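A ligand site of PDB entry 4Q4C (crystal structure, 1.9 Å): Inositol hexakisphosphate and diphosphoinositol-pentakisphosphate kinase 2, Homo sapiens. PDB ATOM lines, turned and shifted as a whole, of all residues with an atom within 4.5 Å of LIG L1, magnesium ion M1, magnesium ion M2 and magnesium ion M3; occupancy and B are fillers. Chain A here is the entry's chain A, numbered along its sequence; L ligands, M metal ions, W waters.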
ATOM      1  N   LYS A  17     -12.306 -14.353  -7.253  1.00  0.00           N
ATOM      2  CA  LYS A  17     -11.477 -15.125  -6.308  1.00  0.00           C
ATOM      3  C   LYS A  17     -11.077 -16.490  -6.875  1.00  0.00           C
ATOM      4  O   LYS A  17      -9.989 -17.010  -6.589  1.00  0.00           O
ATOM      5  CB  LYS A  17     -12.265 -15.318  -5.012  1.00  0.00           C
ATOM      6  CG  LYS A  17     -11.483 -15.887  -3.860  1.00  0.00           C
ATOM      7  CD  LYS A  17     -12.287 -15.740  -2.579  1.00  0.00           C
ATOM      8  CE  LYS A  17     -11.513 -16.324  -1.411  1.00  0.00           C
ATOM      9  NZ  LYS A  17     -12.344 -16.373  -0.188  1.00  0.00           N
ATOM     10  N   LYS A  18     -11.985 -17.086  -7.637  1.00  0.00           N
ATOM     11  CA  LYS A  18     -11.740 -18.379  -8.267  1.00  0.00           C
ATOM     12  C   LYS A  18     -11.149 -18.199  -9.661  1.00  0.00           C
ATOM     13  O   LYS A  18     -10.160 -18.865 -10.003  1.00  0.00           O
ATOM     14  CB  LYS A  18     -13.012 -19.229  -8.310  1.00  0.00           C
ATOM     15  CG  LYS A  18     -13.761 -19.324  -6.975  1.00  0.00           C
ATOM     16  CD  LYS A  18     -12.896 -19.996  -5.909  1.00  0.00           C
ATOM     17  CE  LYS A  18     -13.641 -20.123  -4.590  1.00  0.00           C
ATOM     18  NZ  LYS A  18     -12.811 -20.744  -3.497  1.00  0.00           N
ATOM     19  N   SER A  66     -19.546 -20.336  -5.722  1.00  0.00           N
ATOM     20  CA  SER A  66     -18.794 -20.192  -4.492  1.00  0.00           C
ATOM     21  C   SER A  66     -19.455 -19.004  -3.792  1.00  0.00           C
ATOM     22  O   SER A  66     -20.422 -18.416  -4.323  1.00  0.00           O
ATOM     23  CB  SER A  66     -17.298 -19.929  -4.767  1.00  0.00           C
ATOM     24  OG  SER A  66     -17.117 -18.719  -5.476  1.00  0.00           O
ATOM     25  N   ARG A  98     -25.547 -30.355   2.845  1.00  0.00           N
ATOM     26  CA  ARG A  98     -24.944 -31.660   3.180  1.00  0.00           C
ATOM     27  C   ARG A  98     -25.967 -32.804   3.180  1.00  0.00           C
ATOM     28  O   ARG A  98     -25.623 -33.943   2.858  1.00  0.00           O
ATOM     29  CB  ARG A  98     -24.237 -31.629   4.549  1.00  0.00           C
ATOM     30  CG  ARG A  98     -22.934 -30.858   4.577  1.00  0.00           C
ATOM     31  CD  ARG A  98     -22.256 -30.987   5.941  1.00  0.00           C
ATOM     32  NE  ARG A  98     -21.459 -29.792   6.226  1.00  0.00           N
ATOM     33  CZ  ARG A  98     -20.245 -29.541   5.740  1.00  0.00           C
ATOM     34  NH1 ARG A  98     -19.628 -30.404   4.952  1.00  0.00           N
ATOM     35  NH2 ARG A  98     -19.636 -28.412   6.050  1.00  0.00           N
ATOM     36  N   ALA A 155     -23.417 -26.921   3.651  1.00  0.00           N
ATOM     37  CA  ALA A 155     -22.086 -27.349   3.240  1.00  0.00           C
ATOM     38  C   ALA A 155     -21.079 -26.206   3.139  1.00  0.00           C
ATOM     39  O   ALA A 155     -19.873 -26.412   3.089  1.00  0.00           O
ATOM     40  CB  ALA A 155     -22.157 -28.071   1.916  1.00  0.00           C
ATOM     41  N   HIS A 158     -18.233 -24.354   7.532  1.00  0.00           N
ATOM     42  CA  HIS A 158     -17.136 -25.276   7.833  1.00  0.00           C
ATOM     43  C   HIS A 158     -16.856 -25.455   9.324  1.00  0.00           C
ATOM     44  O   HIS A 158     -15.835 -26.010   9.708  1.00  0.00           O
ATOM     45  CB  HIS A 158     -15.906 -24.817   7.058  1.00  0.00           C
ATOM     46  CG  HIS A 158     -16.173 -24.744   5.596  1.00  0.00           C
ATOM     47  ND1 HIS A 158     -16.347 -25.873   4.829  1.00  0.00           N
ATOM     48  CD2 HIS A 158     -16.446 -23.702   4.793  1.00  0.00           C
ATOM     49  CE1 HIS A 158     -16.669 -25.522   3.596  1.00  0.00           C
ATOM     50  NE2 HIS A 158     -16.731 -24.200   3.552  1.00  0.00           N
ATOM     51  N   ARG A 177     -12.613 -23.034   8.577  1.00  0.00           N
ATOM     52  CA  ARG A 177     -11.752 -22.598   7.485  1.00  0.00           C
ATOM     53  C   ARG A 177     -10.407 -22.124   8.041  1.00  0.00           C
ATOM     54  O   ARG A 177     -10.355 -21.293   8.955  1.00  0.00           O
ATOM     55  CB  ARG A 177     -12.387 -21.439   6.711  1.00  0.00           C
ATOM     56  CG  ARG A 177     -13.275 -21.870   5.586  1.00  0.00           C
ATOM     57  CD  ARG A 177     -12.426 -22.198   4.354  1.00  0.00           C
ATOM     58  NE  ARG A 177     -13.201 -22.873   3.315  1.00  0.00           N
ATOM     59  CZ  ARG A 177     -13.303 -24.210   3.181  1.00  0.00           C
ATOM     60  NH1 ARG A 177     -12.695 -25.042   4.037  1.00  0.00           N
ATOM     61  NH2 ARG A 177     -14.036 -24.712   2.186  1.00  0.00           N
ATOM     62  N   LYS A 178      -9.323 -22.626   7.468  1.00  0.00           N
ATOM     63  CA  LYS A 178      -7.989 -22.322   7.952  1.00  0.00           C
ATOM     64  C   LYS A 178      -7.775 -20.839   8.108  1.00  0.00           C
ATOM     65  O   LYS A 178      -8.186 -20.023   7.251  1.00  0.00           O
ATOM     66  CB  LYS A 178      -6.901 -22.908   7.037  1.00  0.00           C
ATOM     67  CG  LYS A 178      -6.619 -24.376   7.301  1.00  0.00           C
ATOM     68  CD  LYS A 178      -5.676 -24.992   6.268  1.00  0.00           C
ATOM     69  CE  LYS A 178      -6.448 -25.394   5.015  1.00  0.00           C
ATOM     70  NZ  LYS A 178      -5.617 -26.004   3.942  1.00  0.00           N
ATOM     71  N   LYS A 212      -7.808 -36.258  -0.282  1.00  0.00           N
ATOM     72  CA  LYS A 212      -8.508 -35.298  -1.109  1.00  0.00           C
ATOM     73  C   LYS A 212      -8.442 -35.811  -2.554  1.00  0.00           C
ATOM     74  O   LYS A 212      -7.360 -36.066  -3.085  1.00  0.00           O
ATOM     75  CB  LYS A 212      -7.851 -33.918  -1.027  1.00  0.00           C
ATOM     76  CG  LYS A 212      -7.768 -33.286   0.367  1.00  0.00           C
ATOM     77  CD  LYS A 212      -9.090 -32.790   0.881  1.00  0.00           C
ATOM     78  CE  LYS A 212      -9.577 -31.447   0.274  1.00  0.00           C
ATOM     79  NZ  LYS A 212     -10.948 -31.142   0.790  1.00  0.00           N
ATOM     80  N   TYR A 214      -9.703 -35.267  -6.677  1.00  0.00           N
ATOM     81  CA  TYR A 214      -9.980 -34.248  -7.663  1.00  0.00           C
ATOM     82  C   TYR A 214     -10.181 -34.888  -9.014  1.00  0.00           C
ATOM     83  O   TYR A 214      -9.212 -35.390  -9.634  1.00  0.00           O
ATOM     84  CB  TYR A 214      -8.777 -33.303  -7.751  1.00  0.00           C
ATOM     85  CG  TYR A 214      -8.406 -32.582  -6.484  1.00  0.00           C
ATOM     86  CD1 TYR A 214      -8.967 -31.345  -6.194  1.00  0.00           C
ATOM     87  CD2 TYR A 214      -7.503 -33.132  -5.590  1.00  0.00           C
ATOM     88  CE1 TYR A 214      -8.623 -30.665  -5.032  1.00  0.00           C
ATOM     89  CE2 TYR A 214      -7.152 -32.459  -4.425  1.00  0.00           C
ATOM     90  CZ  TYR A 214      -7.716 -31.217  -4.152  1.00  0.00           C
ATOM     91  OH  TYR A 214      -7.375 -30.543  -2.997  1.00  0.00           O
ATOM     92  N   ARG A 226      -3.556 -35.168   3.359  1.00  0.00           N
ATOM     93  CA  ARG A 226      -3.105 -34.137   4.294  1.00  0.00           C
ATOM     94  C   ARG A 226      -3.516 -34.529   5.705  1.00  0.00           C
ATOM     95  O   ARG A 226      -4.450 -35.315   5.903  1.00  0.00           O
ATOM     96  CB  ARG A 226      -3.629 -32.734   3.913  1.00  0.00           C
ATOM     97  CG  ARG A 226      -5.133 -32.611   3.789  1.00  0.00           C
ATOM     98  CD  ARG A 226      -5.762 -31.960   5.016  1.00  0.00           C
ATOM     99  NE  ARG A 226      -7.213 -31.782   4.838  1.00  0.00           N
ATOM    100  CZ  ARG A 226      -7.797 -30.764   4.227  1.00  0.00           C
ATOM    101  NH1 ARG A 226      -7.078 -29.762   3.696  1.00  0.00           N
ATOM    102  NH2 ARG A 226      -9.111 -30.734   4.142  1.00  0.00           N
ATOM    103  N   ARG A 237       2.885 -26.480   6.884  1.00  0.00           N
ATOM    104  CA  ARG A 237       3.116 -25.553   5.774  1.00  0.00           C
ATOM    105  C   ARG A 237       4.516 -25.780   5.209  1.00  0.00           C
ATOM    106  O   ARG A 237       5.444 -26.036   5.958  1.00  0.00           O
ATOM    107  CB  ARG A 237       3.002 -24.102   6.244  1.00  0.00           C
ATOM    108  CG  ARG A 237       1.658 -23.671   6.822  1.00  0.00           C
ATOM    109  CD  ARG A 237       0.686 -23.326   5.704  1.00  0.00           C
ATOM    110  NE  ARG A 237      -0.617 -22.811   6.154  1.00  0.00           N
ATOM    111  CZ  ARG A 237      -1.695 -22.783   5.370  1.00  0.00           C
ATOM    112  NH1 ARG A 237      -1.630 -23.243   4.153  1.00  0.00           N
ATOM    113  NH2 ARG A 237      -2.864 -22.330   5.815  1.00  0.00           N
ATOM    114  N   GLU A 243      -0.003 -25.869   2.135  1.00  0.00           N
ATOM    115  CA  GLU A 243      -0.252 -27.019   3.001  1.00  0.00           C
ATOM    116  C   GLU A 243       0.531 -28.187   2.451  1.00  0.00           C
ATOM    117  O   GLU A 243       0.489 -28.429   1.236  1.00  0.00           O
ATOM    118  CB  GLU A 243      -1.737 -27.364   3.025  1.00  0.00           C
ATOM    119  CG  GLU A 243      -2.089 -28.560   3.876  1.00  0.00           C
ATOM    120  CD  GLU A 243      -3.581 -28.720   4.009  1.00  0.00           C
ATOM    121  OE1 GLU A 243      -4.188 -29.485   3.232  1.00  0.00           O
ATOM    122  OE2 GLU A 243      -4.167 -28.068   4.876  1.00  0.00           O
ATOM    123  N   ARG A 245       1.147 -31.716   1.237  1.00  0.00           N
ATOM    124  CA  ARG A 245       0.333 -32.779   0.658  1.00  0.00           C
ATOM    125  C   ARG A 245       1.176 -34.042   0.393  1.00  0.00           C
ATOM    126  O   ARG A 245       2.322 -33.950  -0.042  1.00  0.00           O
ATOM    127  CB  ARG A 245      -0.334 -32.239  -0.613  1.00  0.00           C
ATOM    128  CG  ARG A 245      -1.357 -31.137  -0.357  1.00  0.00           C
ATOM    129  CD  ARG A 245      -2.597 -31.744   0.298  1.00  0.00           C
ATOM    130  NE  ARG A 245      -3.612 -30.780   0.719  1.00  0.00           N
ATOM    131  CZ  ARG A 245      -4.699 -30.422   0.020  1.00  0.00           C
ATOM    132  NH1 ARG A 245      -4.938 -30.920  -1.186  1.00  0.00           N
ATOM    133  NH2 ARG A 245      -5.551 -29.533   0.544  1.00  0.00           N
ATOM    134  N   ASP A 273     -13.814 -35.716  -0.508  1.00  0.00           N
ATOM    135  CA  ASP A 273     -12.903 -36.162   0.542  1.00  0.00           C
ATOM    136  C   ASP A 273     -13.211 -37.621   0.883  1.00  0.00           C
ATOM    137  O   ASP A 273     -14.408 -38.003   0.993  1.00  0.00           O
ATOM    138  CB  ASP A 273     -13.035 -35.307   1.787  1.00  0.00           C
ATOM    139  CG  ASP A 273     -12.790 -33.815   1.526  1.00  0.00           C
ATOM    140  OD1 ASP A 273     -12.188 -33.428   0.489  1.00  0.00           O
ATOM    141  OD2 ASP A 273     -13.212 -32.992   2.360  1.00  0.00           O
ATOM    142  N   ASP A 285     -17.584 -35.704   2.174  1.00  0.00           N
ATOM    143  CA  ASP A 285     -17.709 -34.329   1.717  1.00  0.00           C
ATOM    144  C   ASP A 285     -17.558 -34.358   0.203  1.00  0.00           C
ATOM    145  O   ASP A 285     -16.670 -35.033  -0.308  1.00  0.00           O
ATOM    146  CB  ASP A 285     -16.608 -33.482   2.367  1.00  0.00           C
ATOM    147  CG  ASP A 285     -16.744 -31.955   2.157  1.00  0.00           C
ATOM    148  OD1 ASP A 285     -17.836 -31.414   1.896  1.00  0.00           O
ATOM    149  OD2 ASP A 285     -15.695 -31.264   2.289  1.00  0.00           O
ATOM    150  N   ASN A 287     -17.411 -31.438  -2.672  1.00  0.00           N
ATOM    151  CA  ASN A 287     -17.356 -29.987  -2.845  1.00  0.00           C
ATOM    152  C   ASN A 287     -17.659 -29.445  -4.244  1.00  0.00           C
ATOM    153  O   ASN A 287     -17.891 -28.242  -4.392  1.00  0.00           O
ATOM    154  CB  ASN A 287     -15.995 -29.518  -2.373  1.00  0.00           C
ATOM    155  CG  ASN A 287     -15.777 -29.812  -0.912  1.00  0.00           C
ATOM    156  OD1 ASN A 287     -16.587 -29.407  -0.060  1.00  0.00           O
ATOM    157  ND2 ASN A 287     -14.700 -30.505  -0.601  1.00  0.00           N
ATOM    158  N   PHE A 289     -16.644 -28.078  -7.918  1.00  0.00           N
ATOM    159  CA  PHE A 289     -15.486 -27.563  -8.640  1.00  0.00           C
ATOM    160  C   PHE A 289     -14.340 -27.175  -7.711  1.00  0.00           C
ATOM    161  O   PHE A 289     -14.479 -26.296  -6.866  1.00  0.00           O
ATOM    162  CB  PHE A 289     -15.861 -26.344  -9.478  1.00  0.00           C
ATOM    163  CG  PHE A 289     -14.906 -26.060 -10.593  1.00  0.00           C
ATOM    164  CD1 PHE A 289     -13.671 -25.489 -10.344  1.00  0.00           C
ATOM    165  CD2 PHE A 289     -15.252 -26.370 -11.897  1.00  0.00           C
ATOM    166  CE1 PHE A 289     -12.798 -25.200 -11.400  1.00  0.00           C
ATOM    167  CE2 PHE A 289     -14.400 -26.112 -12.947  1.00  0.00           C
ATOM    168  CZ  PHE A 289     -13.171 -25.533 -12.701  1.00  0.00           C
ATOM    169  N   SER A 290     -13.217 -27.867  -7.870  1.00  0.00           N
ATOM    170  CA  SER A 290     -11.999 -27.631  -7.119  1.00  0.00           C
ATOM    171  C   SER A 290     -10.792 -28.081  -7.977  1.00  0.00           C
ATOM    172  O   SER A 290     -10.824 -29.147  -8.610  1.00  0.00           O
ATOM    173  CB  SER A 290     -12.035 -28.381  -5.759  1.00  0.00           C
ATOM    174  OG  SER A 290     -10.874 -28.101  -4.979  1.00  0.00           O
ATOM    175  N   LYS A 293      -3.888 -27.370  -6.108  1.00  0.00           N
ATOM    176  CA  LYS A 293      -2.881 -26.321  -6.023  1.00  0.00           C
ATOM    177  C   LYS A 293      -1.487 -27.020  -6.127  1.00  0.00           C
ATOM    178  O   LYS A 293      -1.280 -28.102  -5.605  1.00  0.00           O
ATOM    179  CB  LYS A 293      -3.033 -25.536  -4.698  1.00  0.00           C
ATOM    180  CG  LYS A 293      -4.443 -24.942  -4.433  1.00  0.00           C
ATOM    181  CD  LYS A 293      -4.543 -24.234  -3.065  1.00  0.00           C
ATOM    182  CE  LYS A 293      -5.974 -24.078  -2.565  1.00  0.00           C
ATOM    183  NZ  LYS A 293      -6.124 -23.502  -1.191  1.00  0.00           N
HETATM  184  C1  LIG L   1     -11.138 -25.369  -0.073  1.00  0.00           C
HETATM  185  C2  LIG L   1     -11.847 -24.278  -0.910  1.00  0.00           C
HETATM  186  C3  LIG L   1     -11.919 -22.982  -0.083  1.00  0.00           C
HETATM  187  C4  LIG L   1     -10.505 -22.476   0.227  1.00  0.00           C
HETATM  188  C5  LIG L   1      -9.689 -23.551   0.964  1.00  0.00           C
HETATM  189  C6  LIG L   1      -9.693 -24.941   0.288  1.00  0.00           C
HETATM  190  O1  LIG L   1     -11.089 -26.582  -0.823  1.00  0.00           O
HETATM  191  O2  LIG L   1     -11.077 -24.053  -2.089  1.00  0.00           O
HETATM  192  O3  LIG L   1     -12.706 -21.972  -0.765  1.00  0.00           O
HETATM  193  O4  LIG L   1     -10.557 -21.392   1.153  1.00  0.00           O
HETATM  194  O5  LIG L   1      -8.331 -23.130   1.027  1.00  0.00           O
HETATM  195  O6  LIG L   1      -9.152 -25.851   1.278  1.00  0.00           O
HETATM  196  O7  LIG L   1     -11.577 -29.010  -0.860  1.00  0.00           O
HETATM  197  O8  LIG L   1     -12.526 -25.738  -3.386  1.00  0.00           O
HETATM  198  O9  LIG L   1     -13.821 -20.864   1.122  1.00  0.00           O
HETATM  199  O10 LIG L   1     -11.959 -19.292   0.769  1.00  0.00           O
HETATM  200  O11 LIG L   1      -7.404 -21.026   2.102  1.00  0.00           O
HETATM  201  O12 LIG L   1      -6.994 -26.070   0.100  1.00  0.00           O
HETATM  202  O13 LIG L   1     -13.217 -27.270  -1.692  1.00  0.00           O
HETATM  203  O14 LIG L   1     -10.592 -24.621  -4.389  1.00  0.00           O
HETATM  204  O15 LIG L   1     -14.673 -20.624  -1.216  1.00  0.00           O
HETATM  205  O16 LIG L   1      -9.758 -19.664  -0.491  1.00  0.00           O
HETATM  206  O17 LIG L   1      -8.558 -22.781   3.590  1.00  0.00           O
HETATM  207  O18 LIG L   1      -8.569 -28.036   0.411  1.00  0.00           O
HETATM  208  O19 LIG L   1     -12.911 -27.485   0.801  1.00  0.00           O
HETATM  209  O20 LIG L   1     -12.583 -23.324  -3.791  1.00  0.00           O
HETATM  210  O21 LIG L   1     -14.851 -22.814   0.030  1.00  0.00           O
HETATM  211  O22 LIG L   1      -9.816 -19.174   1.994  1.00  0.00           O
HETATM  212  O23 LIG L   1      -6.332 -23.286   2.470  1.00  0.00           O
HETATM  213  O24 LIG L   1      -7.370 -27.129   2.335  1.00  0.00           O
HETATM  214  O25 LIG L   1     -13.038 -29.992   2.001  1.00  0.00           O
HETATM  215  O26 LIG L   1      -3.930 -23.945   2.756  1.00  0.00           O
HETATM  216  O27 LIG L   1     -15.152 -28.240   2.082  1.00  0.00           O
HETATM  217  O28 LIG L   1      -4.720 -21.692   3.598  1.00  0.00           O
HETATM  218  O29 LIG L   1     -12.871 -27.784   3.351  1.00  0.00           O
HETATM  219  O30 LIG L   1      -4.545 -22.087   1.109  1.00  0.00           O
HETATM  220  P1  LIG L   1     -12.261 -27.708  -0.653  1.00  0.00           P
HETATM  221  P2  LIG L   1     -11.731 -24.468  -3.530  1.00  0.00           P
HETATM  222  P3  LIG L   1     -14.135 -21.521  -0.155  1.00  0.00           P
HETATM  223  P4  LIG L   1     -10.423 -19.809   0.810  1.00  0.00           P
HETATM  224  P5  LIG L   1      -7.711 -22.442   2.407  1.00  0.00           P
HETATM  225  P6  LIG L   1      -7.884 -26.842   0.977  1.00  0.00           P
HETATM  226  P7  LIG L   1     -13.472 -28.416   2.093  1.00  0.00           P
HETATM  227  P8  LIG L   1      -4.845 -22.625   2.471  1.00  0.00           P
HETATM  228  P1  LG2 L   2     -15.995 -29.440   5.123  1.00  0.00           P
HETATM  229  O1  LG2 L   2     -17.094 -29.430   4.075  1.00  0.00           O
HETATM  230  O2  LG2 L   2     -16.109 -28.332   6.109  1.00  0.00           O
HETATM  231  O3  LG2 L   2     -14.604 -29.615   4.532  1.00  0.00           O
HETATM  232  P2  LG2 L   2     -15.870 -32.218   5.977  1.00  0.00           P
HETATM  233  O4  LG2 L   2     -17.065 -33.145   6.019  1.00  0.00           O
HETATM  234  O5  LG2 L   2     -14.821 -32.429   4.946  1.00  0.00           O
HETATM  235  O6  LG2 L   2     -16.364 -30.693   6.083  1.00  0.00           O
HETATM  236  O7  LG2 L   2     -15.209 -32.363   7.443  1.00  0.00           O
HETATM  237  C1  LG2 L   2     -13.997 -31.678   7.771  1.00  0.00           C
HETATM  238  C2  LG2 L   2     -12.941 -32.677   8.222  1.00  0.00           C
HETATM  239  O8  LG2 L   2     -13.394 -33.359   9.386  1.00  0.00           O
HETATM  240  C3  LG2 L   2     -12.641 -33.793   7.245  1.00  0.00           C
HETATM  241  O9  LG2 L   2     -11.670 -33.458   6.245  1.00  0.00           O
HETATM  242  C4  LG2 L   2     -12.137 -34.906   8.146  1.00  0.00           C
HETATM  243  O10 LG2 L   2     -10.769 -34.724   8.606  1.00  0.00           O
HETATM  244  C5  LG2 L   2     -13.029 -34.743   9.355  1.00  0.00           C
HETATM  245  N1  LG2 L   2     -14.257 -35.564   9.282  1.00  0.00           N
HETATM  246  C6  LG2 L   2     -15.452 -35.257   8.739  1.00  0.00           C
HETATM  247  N2  LG2 L   2     -16.344 -36.281   8.898  1.00  0.00           N
HETATM  248  C7  LG2 L   2     -15.669 -37.254   9.543  1.00  0.00           C
HETATM  249  C8  LG2 L   2     -15.990 -38.592  10.061  1.00  0.00           C
HETATM  250  N3  LG2 L   2     -17.217 -39.099   9.879  1.00  0.00           N
HETATM  251  N4  LG2 L   2     -15.027 -39.289  10.683  1.00  0.00           N
HETATM  252  C9  LG2 L   2     -13.799 -38.782  10.866  1.00  0.00           C
HETATM  253  N5  LG2 L   2     -13.431 -37.571  10.418  1.00  0.00           N
HETATM  254  C10 LG2 L   2     -14.320 -36.777   9.794  1.00  0.00           C
HETATM  255 MG    MG M   1     -16.833 -29.379   2.000  1.00  0.00          MG
HETATM  256 MG    MG M   2     -13.844 -31.370   3.468  1.00  0.00          MG
HETATM  257 MG    MG M   3      -8.059 -19.317   3.092  1.00  0.00          MG
HETATM  258 MG    MG M   4     -16.955 -24.671  -3.320  1.00  0.00          MG
HETATM  259  O   HOH W   1     -12.598 -30.658  -2.682  1.00  0.00           O
HETATM  260  O   HOH W   2      -9.866 -24.499   5.208  1.00  0.00           O
HETATM  261  O   HOH W   3      -8.464 -17.498   4.090  1.00  0.00           O
HETATM  262  O   HOH W   4      -8.603 -26.070  -3.112  1.00  0.00           O
HETATM  263  O   HOH W   5     -11.640 -28.965   5.516  1.00  0.00           O
HETATM  264  O   HOH W   6      -4.309 -26.075   0.679  1.00  0.00           O
HETATM  265  O   HOH W   7      -2.208 -22.564  -0.327  1.00  0.00           O
HETATM  266  O   HOH W   8     -17.368 -20.716  -1.493  1.00  0.00           O
HETATM  267  O   HOH W   9     -11.948 -31.452   4.402  1.00  0.00           O
HETATM  268  O   HOH W  10      -6.946 -18.158   1.650  1.00  0.00           O
HETATM  269  O   HOH W  11     -10.664 -28.919   2.215  1.00  0.00           O
HETATM  270  O   HOH W  12      -4.765 -19.489   0.688  1.00  0.00           O
HETATM  271  O   HOH W  13     -10.570 -19.412  -2.924  1.00  0.00           O
HETATM  272  O   HOH W  14     -17.377 -23.002   1.140  1.00  0.00           O
HETATM  273  O   HOH W  15      -9.081 -20.367   4.623  1.00  0.00           O
HETATM  274  O   HOH W  16     -15.204 -23.870  -2.427  1.00  0.00           O
HETATM  275  O   HOH W  17      -6.209 -19.555   4.202  1.00  0.00           O
HETATM  276  O   HOH W  18     -18.336 -28.166   1.656  1.00  0.00           O
HETATM  277  O   HOH W  19     -14.962 -18.056  -1.555  1.00  0.00           O
HETATM  278  O   HOH W  20      -9.018 -28.457  -2.272  1.00  0.00           O
HETATM  279  O   HOH W  21      -8.378 -17.309  -0.510  1.00  0.00           O
HETATM  280  O   HOH W  22      -7.434 -21.057  -1.039  1.00  0.00           O
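The side-chain amino group (NZ) of Lys 18 is in salt-bridge range of an oxygen (O20) of LIG L1 (2.6 Å).
The side-chain amino group (NZ) of Lys 178 lies within salt-bridge range of an oxygen (O24) of LIG L1 (2.6 Å).
NZ of Lys 212 is in salt-bridge range of O7 of LIG L1 (2.8 Å).
The guanidinium group (NH1) of Arg 237 is in salt-bridge range of an oxygen (O26) of LIG L1.
O29 of LIG L1 is in salt-bridge range of NH1 of Arg 177 (2.8 Å).
O24 of LIG L1 lies within salt-bridge range of NH1 of Arg 226 (3.0 Å).
The side-chain amino group (NZ) of Lys 293 lies within salt-bridge range of an oxygen (O12) of LIG L1 (3.0 Å).
The side-chain amino group (NZ) of Lys 17 is in salt-bridge range of an oxygen (O10) of LIG L1, at 3.1 Å.
An oxygen (O8) of LIG L1 sits at hydrogen-bond distance from the side-chain hydroxyl of Ser 290 (3.3 Å).
The guanidinium group of Arg 245 is in salt-bridge range of an oxygen (O18) of LIG L1.
ND1 of His 158 sits at hydrogen-bond distance from O2 of LG2 L2, 2.8 Å away.
O2 of LG2 L2 is in salt-bridge range of NH2 of Arg 98, at 3.5 Å.
OD1 of Asp 273 lies within salt-bridge range of NZ of Lys 212.
OD1 of Asp 285 sits close to NH1 of Arg 98 (3.7 Å).
The side-chain amino group (NZ) of Lys 178 is in salt-bridge range of the side-chain carboxylate (OE2) of Glu 243 (2.7 Å).
The guanidinium group (NH2) of Arg 177 lies within hydrogen-bond range of a ring nitrogen (NE2) of His 158, 3.1 Å away.
OE1 of Glu 243 is in salt-bridge range of NH1 of Arg 226, 2.9 Å away.
OE1 of Glu 243 lies within salt-bridge range of NE of Arg 245 (2.9 Å).
The guanidinium group of Arg 245 lies within hydrogen-bond range of the side-chain hydroxyl of Tyr 214, at 3.1 Å.
Residues that only touch LIG L1: His 158.
Of the 20 residues printed, 14 come within 4 Å of LIG L1.
The nearest printed residue that does not touch LIG L1 is Phe 289 (4.03 Å).
Two residues have an atom within 4 Å of magnesium ion M1: Asp 285 and Asn 287.
Lys 212 touches magnesium ion M2.
Of the 20 residues printed, 3 come within 4 Å of magnesium ion M2.
Along chain A the residues within 4 Å of magnesium ion M2 span positions 212 to 285.
The nearest printed residue that does not touch magnesium ion M2 is Asn 287 (4.2 Å).
No residue comes within 4 Å of magnesium ion M3.
Magnesium ion M1 is bound by water W18 (2.0 Å), an oxygen (O27) of LIG L1 (2.0 Å), the side-chain amide oxygen (OD1) of Asn 287 (2.1 Å), an oxygen (O1) of LG2 L2 (2.1 Å), the side-chain carboxylate (OD2) of Asp 285 (2.2 Å) and the side-chain carboxylate (OD1) of Asp 285 (2.3 Å).
Magnesium ion M2 is bound by OD2 of Asp 273, O5 of LG2 L2, water W9, O25 of LIG L1, O3 of LG2 L2 and OD2 of Asp 285.
Magnesium ion M2 has six donor atoms within binding distance.
Magnesium ion M3 is bound by an oxygen (O22) of LIG L1 (2.1 Å), an oxygen (O11) of LIG L1 (2.1 Å), water W3 (2.1 Å), water W15 (2.1 Å), water W10 (2.2 Å) and water W17 (2.2 Å).
Water W15 bridges O17 of LIG L1 and O of Lys 178.
Water W1 lies within hydrogen-bond range of O7 of LIG L1 and ND2 of Asn 287.
Water W2 lies within hydrogen-bond range of O17 of LIG L1, N of Lys 178 and NH1 of Arg 177.
Water W5 bridges an oxygen (O29) of LIG L1 and the guanidinium group of Arg 226.
Water W22 lies within hydrogen-bond range of O16 of LIG L1 (2.8 Å) and NZ of Lys 293 (2.8 Å).
Water W14 lies within hydrogen-bond range of an oxygen (O21) of LIG L1 and a ring nitrogen (NE2) of His 158.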
